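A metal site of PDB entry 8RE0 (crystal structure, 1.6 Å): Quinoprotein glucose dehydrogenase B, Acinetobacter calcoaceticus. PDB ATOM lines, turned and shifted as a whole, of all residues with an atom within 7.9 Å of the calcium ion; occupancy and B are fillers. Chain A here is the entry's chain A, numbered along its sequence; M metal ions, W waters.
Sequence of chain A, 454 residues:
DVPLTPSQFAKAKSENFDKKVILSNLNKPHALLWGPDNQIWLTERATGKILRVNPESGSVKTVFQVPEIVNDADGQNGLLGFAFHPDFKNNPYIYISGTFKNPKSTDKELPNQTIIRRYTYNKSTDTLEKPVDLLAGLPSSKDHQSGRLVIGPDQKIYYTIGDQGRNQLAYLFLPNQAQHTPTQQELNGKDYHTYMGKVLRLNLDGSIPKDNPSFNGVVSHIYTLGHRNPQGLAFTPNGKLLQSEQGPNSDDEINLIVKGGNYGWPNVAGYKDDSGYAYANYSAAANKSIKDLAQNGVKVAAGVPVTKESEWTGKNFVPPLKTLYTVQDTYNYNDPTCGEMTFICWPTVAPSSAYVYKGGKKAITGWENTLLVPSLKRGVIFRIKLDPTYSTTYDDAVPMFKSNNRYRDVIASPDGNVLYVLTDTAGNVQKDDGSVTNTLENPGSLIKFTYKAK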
ATOM      1  N   SER A 250      12.809 -33.051  13.089  1.00  0.00           N
ATOM      2  CA  SER A 250      13.456 -32.557  11.893  1.00  0.00           C
ATOM      3  C   SER A 250      14.924 -32.926  11.976  1.00  0.00           C
ATOM      4  O   SER A 250      15.397 -33.422  13.001  1.00  0.00           O
ATOM      5  CB  SER A 250      13.310 -31.050  11.774  1.00  0.00           C
ATOM      6  OG  SER A 250      14.050 -30.453  12.796  1.00  0.00           O
ATOM      7  N   ASP A 251      15.642 -32.640  10.892  1.00  0.00           N
ATOM      8  CA  ASP A 251      17.107 -32.605  10.903  1.00  0.00           C
ATOM      9  C   ASP A 251      17.753 -33.914  11.355  1.00  0.00           C
ATOM     10  O   ASP A 251      18.721 -33.904  12.133  1.00  0.00           O
ATOM     11  CB  ASP A 251      17.613 -31.451  11.764  1.00  0.00           C
ATOM     12  CG  ASP A 251      17.249 -30.105  11.210  1.00  0.00           C
ATOM     13  OD1 ASP A 251      17.981 -29.668  10.294  1.00  0.00           O
ATOM     14  OD2 ASP A 251      16.298 -29.457  11.739  1.00  0.00           O
ATOM     15  N   GLU A 253      20.601 -36.382  10.311  1.00  0.00           N
ATOM     16  CA  GLU A 253      21.894 -35.929   9.811  1.00  0.00           C
ATOM     17  C   GLU A 253      22.726 -37.049   9.186  1.00  0.00           C
ATOM     18  O   GLU A 253      22.716 -38.203   9.649  1.00  0.00           O
ATOM     19  CB  GLU A 253      22.735 -35.299  10.951  1.00  0.00           C
ATOM     20  CG  GLU A 253      22.141 -34.019  11.540  1.00  0.00           C
ATOM     21  CD  GLU A 253      22.925 -33.491  12.712  1.00  0.00           C
ATOM     22  OE1 GLU A 253      23.803 -34.221  13.232  1.00  0.00           O
ATOM     23  OE2 GLU A 253      22.664 -32.342  13.106  1.00  0.00           O
ATOM     24  N   ASN A 267      21.738 -28.376  21.629  1.00  0.00           N
ATOM     25  CA  ASN A 267      21.604 -26.943  21.365  1.00  0.00           C
ATOM     26  C   ASN A 267      21.364 -26.653  19.892  1.00  0.00           C
ATOM     27  O   ASN A 267      20.735 -25.641  19.568  1.00  0.00           O
ATOM     28  CB  ASN A 267      22.844 -26.221  21.871  1.00  0.00           C
ATOM     29  CG  ASN A 267      22.987 -26.332  23.362  1.00  0.00           C
ATOM     30  OD1 ASN A 267      23.583 -27.292  23.873  1.00  0.00           O
ATOM     31  ND2 ASN A 267      22.413 -25.370  24.086  1.00  0.00           N
ATOM     32  N   VAL A 268      21.814 -27.530  19.009  1.00  0.00           N
ATOM     33  CA  VAL A 268      21.709 -27.337  17.560  1.00  0.00           C
ATOM     34  C   VAL A 268      21.259 -28.636  16.929  1.00  0.00           C
ATOM     35  O   VAL A 268      21.882 -29.676  17.147  1.00  0.00           O
ATOM     36  CB  VAL A 268      23.023 -26.873  16.905  1.00  0.00           C
ATOM     37  CG1 VAL A 268      22.787 -26.541  15.428  1.00  0.00           C
ATOM     38  CG2 VAL A 268      23.610 -25.629  17.609  1.00  0.00           C
ATOM     39  N   ALA A 269      20.112 -28.599  16.245  1.00  0.00           N
ATOM     40  CA  ALA A 269      19.677 -29.701  15.381  1.00  0.00           C
ATOM     41  C   ALA A 269      20.011 -29.377  13.922  1.00  0.00           C
ATOM     42  O   ALA A 269      19.536 -28.375  13.374  1.00  0.00           O
ATOM     43  CB  ALA A 269      18.179 -29.932  15.561  1.00  0.00           C
ATOM     44  N   GLY A 270      20.846 -30.213  13.300  1.00  0.00           N
ATOM     45  CA  GLY A 270      21.209 -29.947  11.923  1.00  0.00           C
ATOM     46  C   GLY A 270      22.149 -28.755  11.847  1.00  0.00           C
ATOM     47  O   GLY A 270      23.135 -28.639  12.595  1.00  0.00           O
ATOM     48  N   TYR A 271      21.894 -27.874  10.876  1.00  0.00           N
ATOM     49  CA  TYR A 271      22.700 -26.680  10.736  1.00  0.00           C
ATOM     50  C   TYR A 271      22.376 -25.714  11.875  1.00  0.00           C
ATOM     51  O   TYR A 271      21.301 -25.774  12.480  1.00  0.00           O
ATOM     52  CB  TYR A 271      22.421 -25.969   9.402  1.00  0.00           C
ATOM     53  CG  TYR A 271      22.699 -26.860   8.208  1.00  0.00           C
ATOM     54  CD1 TYR A 271      23.991 -27.043   7.736  1.00  0.00           C
ATOM     55  CD2 TYR A 271      21.685 -27.528   7.587  1.00  0.00           C
ATOM     56  CE1 TYR A 271      24.271 -27.914   6.684  1.00  0.00           C
ATOM     57  CE2 TYR A 271      21.925 -28.392   6.514  1.00  0.00           C
ATOM     58  CZ  TYR A 271      23.222 -28.560   6.058  1.00  0.00           C
ATOM     59  OH  TYR A 271      23.428 -29.393   5.031  1.00  0.00           O
ATOM     60  N   LYS A 272      23.301 -24.799  12.146  1.00  0.00           N
ATOM     61  CA  LYS A 272      23.056 -23.690  13.088  1.00  0.00           C
ATOM     62  C   LYS A 272      22.375 -22.579  12.305  1.00  0.00           C
ATOM     63  O   LYS A 272      22.970 -21.564  11.917  1.00  0.00           O
ATOM     64  CB  LYS A 272      24.341 -23.217  13.724  1.00  0.00           C
ATOM     65  CG  LYS A 272      24.155 -22.360  14.944  1.00  0.00           C
ATOM     66  CD  LYS A 272      25.433 -21.662  15.339  1.00  0.00           C
ATOM     67  CE  LYS A 272      26.324 -22.559  16.196  1.00  0.00           C
ATOM     68  NZ  LYS A 272      27.408 -21.750  16.834  1.00  0.00           N
ATOM     69  N   ASP A 273      21.087 -22.806  12.028  1.00  0.00           N
ATOM     70  CA  ASP A 273      20.285 -21.962  11.150  1.00  0.00           C
ATOM     71  C   ASP A 273      19.082 -21.293  11.811  1.00  0.00           C
ATOM     72  O   ASP A 273      18.381 -20.527  11.144  1.00  0.00           O
ATOM     73  CB  ASP A 273      19.803 -22.758   9.922  1.00  0.00           C
ATOM     74  CG  ASP A 273      19.098 -24.060  10.285  1.00  0.00           C
ATOM     75  OD1 ASP A 273      18.707 -24.314  11.436  1.00  0.00           O
ATOM     76  OD2 ASP A 273      18.882 -24.875   9.372  1.00  0.00           O
ATOM     77  N   ASP A 274      18.772 -21.603  13.070  1.00  0.00           N
ATOM     78  CA  ASP A 274      17.541 -21.107  13.700  1.00  0.00           C
ATOM     79  C   ASP A 274      16.302 -21.385  12.851  1.00  0.00           C
ATOM     80  O   ASP A 274      15.363 -20.590  12.813  1.00  0.00           O
ATOM     81  CB  ASP A 274      17.630 -19.607  14.012  1.00  0.00           C
ATOM     82  CG  ASP A 274      18.631 -19.254  15.090  1.00  0.00           C
ATOM     83  OD1 ASP A 274      19.243 -20.157  15.729  1.00  0.00           O
ATOM     84  OD2 ASP A 274      18.805 -18.031  15.356  1.00  0.00           O
ATOM     85  N   SER A 275      16.268 -22.530  12.192  1.00  0.00           N
ATOM     86  CA  SER A 275      15.206 -22.888  11.250  1.00  0.00           C
ATOM     87  C   SER A 275      14.522 -24.190  11.632  1.00  0.00           C
ATOM     88  O   SER A 275      15.068 -25.263  11.377  1.00  0.00           O
ATOM     89  CB  SER A 275      15.762 -22.983   9.827  1.00  0.00           C
ATOM     90  OG  SER A 275      14.734 -22.883   8.865  1.00  0.00           O
ATOM     91  N   GLY A 276      13.306 -24.085  12.178  1.00  0.00           N
ATOM     92  CA  GLY A 276      12.454 -25.211  12.447  1.00  0.00           C
ATOM     93  C   GLY A 276      12.730 -25.967  13.723  1.00  0.00           C
ATOM     94  O   GLY A 276      12.063 -26.996  13.951  1.00  0.00           O
ATOM     95  N   TYR A 277      13.685 -25.506  14.541  1.00  0.00           N
ATOM     96  CA  TYR A 277      14.023 -26.116  15.812  1.00  0.00           C
ATOM     97  C   TYR A 277      14.555 -25.032  16.749  1.00  0.00           C
ATOM     98  O   TYR A 277      15.200 -24.087  16.319  1.00  0.00           O
ATOM     99  CB  TYR A 277      15.108 -27.180  15.679  1.00  0.00           C
ATOM    100  CG  TYR A 277      15.616 -27.755  16.997  1.00  0.00           C
ATOM    101  CD1 TYR A 277      14.908 -28.787  17.667  1.00  0.00           C
ATOM    102  CD2 TYR A 277      16.793 -27.294  17.561  1.00  0.00           C
ATOM    103  CE1 TYR A 277      15.382 -29.321  18.856  1.00  0.00           C
ATOM    104  CE2 TYR A 277      17.304 -27.844  18.742  1.00  0.00           C
ATOM    105  CZ  TYR A 277      16.568 -28.837  19.400  1.00  0.00           C
ATOM    106  OH  TYR A 277      17.057 -29.363  20.564  1.00  0.00           O
ATOM    107  N   ALA A 278      14.328 -25.222  18.044  1.00  0.00           N
ATOM    108  CA  ALA A 278      15.009 -24.458  19.085  1.00  0.00           C
ATOM    109  C   ALA A 278      15.133 -25.385  20.276  1.00  0.00           C
ATOM    110  O   ALA A 278      14.419 -26.382  20.369  1.00  0.00           O
ATOM    111  CB  ALA A 278      14.254 -23.176  19.474  1.00  0.00           C
ATOM    112  N   ASN A 296       8.892 -29.126  18.211  1.00  0.00           N
ATOM    113  CA  ASN A 296      10.319 -28.991  17.922  1.00  0.00           C
ATOM    114  C   ASN A 296      10.923 -27.739  18.546  1.00  0.00           C
ATOM    115  O   ASN A 296      11.961 -27.253  18.067  1.00  0.00           O
ATOM    116  CB  ASN A 296      10.582 -29.023  16.416  1.00  0.00           C
ATOM    117  CG  ASN A 296      11.736 -29.948  16.066  1.00  0.00           C
ATOM    118  OD1 ASN A 296      11.946 -30.999  16.708  1.00  0.00           O
ATOM    119  ND2 ASN A 296      12.466 -29.591  15.031  1.00  0.00           N
ATOM    120  N   GLU A 309      19.420 -21.760  18.366  1.00  0.00           N
ATOM    121  CA  GLU A 309      20.682 -22.353  17.951  1.00  0.00           C
ATOM    122  C   GLU A 309      21.801 -21.312  17.914  1.00  0.00           C
ATOM    123  O   GLU A 309      22.919 -21.579  18.363  1.00  0.00           O
ATOM    124  CB  GLU A 309      20.471 -22.998  16.581  1.00  0.00           C
ATOM    125  CG  GLU A 309      19.469 -24.156  16.629  1.00  0.00           C
ATOM    126  CD  GLU A 309      19.289 -24.859  15.287  1.00  0.00           C
ATOM    127  OE1 GLU A 309      19.287 -24.171  14.237  1.00  0.00           O
ATOM    128  OE2 GLU A 309      19.122 -26.121  15.301  1.00  0.00           O
ATOM    129  N   PHE A 317      31.997 -26.719  17.115  1.00  0.00           N
ATOM    130  CA  PHE A 317      30.750 -27.145  16.491  1.00  0.00           C
ATOM    131  C   PHE A 317      30.975 -27.521  15.028  1.00  0.00           C
ATOM    132  O   PHE A 317      31.468 -26.692  14.247  1.00  0.00           O
ATOM    133  CB  PHE A 317      29.672 -26.066  16.554  1.00  0.00           C
ATOM    134  CG  PHE A 317      28.473 -26.438  15.735  1.00  0.00           C
ATOM    135  CD1 PHE A 317      27.744 -27.576  16.030  1.00  0.00           C
ATOM    136  CD2 PHE A 317      28.095 -25.680  14.628  1.00  0.00           C
ATOM    137  CE1 PHE A 317      26.642 -27.967  15.253  1.00  0.00           C
ATOM    138  CE2 PHE A 317      27.009 -26.060  13.834  1.00  0.00           C
ATOM    139  CZ  PHE A 317      26.266 -27.203  14.164  1.00  0.00           C
ATOM    140  N   PRO A 320      26.369 -30.796   9.963  1.00  0.00           N
ATOM    141  CA  PRO A 320      26.212 -32.008   9.136  1.00  0.00           C
ATOM    142  C   PRO A 320      26.556 -31.776   7.656  1.00  0.00           C
ATOM    143  O   PRO A 320      26.434 -30.676   7.107  1.00  0.00           O
ATOM    144  CB  PRO A 320      24.728 -32.348   9.313  1.00  0.00           C
ATOM    145  CG  PRO A 320      24.101 -30.992   9.546  1.00  0.00           C
ATOM    146  CD  PRO A 320      25.084 -30.184  10.321  1.00  0.00           C
ATOM    147  N   THR A 323      21.239 -32.795   5.803  1.00  0.00           N
ATOM    148  CA  THR A 323      20.117 -33.015   6.706  1.00  0.00           C
ATOM    149  C   THR A 323      18.935 -33.632   5.974  1.00  0.00           C
ATOM    150  O   THR A 323      18.618 -33.249   4.838  1.00  0.00           O
ATOM    151  CB  THR A 323      19.622 -31.719   7.344  1.00  0.00           C
ATOM    152  OG1 THR A 323      19.304 -30.781   6.316  1.00  0.00           O
ATOM    153  CG2 THR A 323      20.694 -31.149   8.315  1.00  0.00           C
ATOM    154  N   THR A 326      15.495 -30.333   6.587  1.00  0.00           N
ATOM    155  CA  THR A 326      15.462 -29.047   7.253  1.00  0.00           C
ATOM    156  C   THR A 326      14.288 -28.258   6.694  1.00  0.00           C
ATOM    157  O   THR A 326      14.082 -28.232   5.474  1.00  0.00           O
ATOM    158  CB  THR A 326      16.757 -28.278   7.066  1.00  0.00           C
ATOM    159  OG1 THR A 326      17.823 -29.038   7.656  1.00  0.00           O
ATOM    160  CG2 THR A 326      16.688 -26.911   7.760  1.00  0.00           C
ATOM    161  N   VAL A 327      13.522 -27.641   7.603  1.00  0.00           N
ATOM    162  CA  VAL A 327      12.359 -26.859   7.237  1.00  0.00           C
ATOM    163  C   VAL A 327      12.404 -25.473   7.882  1.00  0.00           C
ATOM    164  O   VAL A 327      13.232 -25.187   8.743  1.00  0.00           O
ATOM    165  CB  VAL A 327      11.058 -27.588   7.635  1.00  0.00           C
ATOM    166  CG1 VAL A 327      10.902 -28.911   6.870  1.00  0.00           C
ATOM    167  CG2 VAL A 327      11.012 -27.783   9.140  1.00  0.00           C
HETATM  168 CA    CA M   1      19.096 -26.156  12.829  1.00  0.00          CA
HETATM  169  O   HOH W   1      19.120 -27.240  10.510  1.00  0.00           O
HETATM  170  O   HOH W   2      16.803 -26.804  12.770  1.00  0.00           O
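The backbone NH (N) of Ser 275 sits close to the side-chain carboxylate (OD1) of Asp 273, at 3.1 Å.
The backbone NH (N) of Glu 309 lies within hydrogen-bond range of the side-chain carboxylate (OD1) of Asp 274, at 3.1 Å.
Within 4 Å of the calcium ion: Ala 269, Tyr 271, Asp 273 and Glu 309.
The nearest printed residue that does not touch the calcium ion is Gly 270 (4.1 Å).
The calcium ion is bound by the backbone carbonyl oxygen (O) of Tyr 271 (2.3 Å), the backbone carbonyl oxygen (O) of Ala 269 (2.3 Å), the side-chain carboxylate (OD1) of Asp 273 (2.3 Å), water W2 (2.4 Å), the side-chain carboxylate (OE1) of Glu 309 (2.4 Å), the side-chain carboxylate (OE2) of Glu 309 (2.5 Å) and water W1 (2.6 Å).
The calcium ion has seven donor atoms within binding distance.
Water W1 lies within hydrogen-bond range of the side-chain carboxylate (OD2) of Asp 273 (2.6 Å), the side-chain carboxylate (OD1) of Asp 251 (2.7 Å) and the backbone NH (N) of Tyr 271 (2.9 Å).
Water W2 bridges the backbone carbonyl oxygen of Ser 275 (2.7 Å) and the side-chain carboxylate of Asp 251 (2.9 Å).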
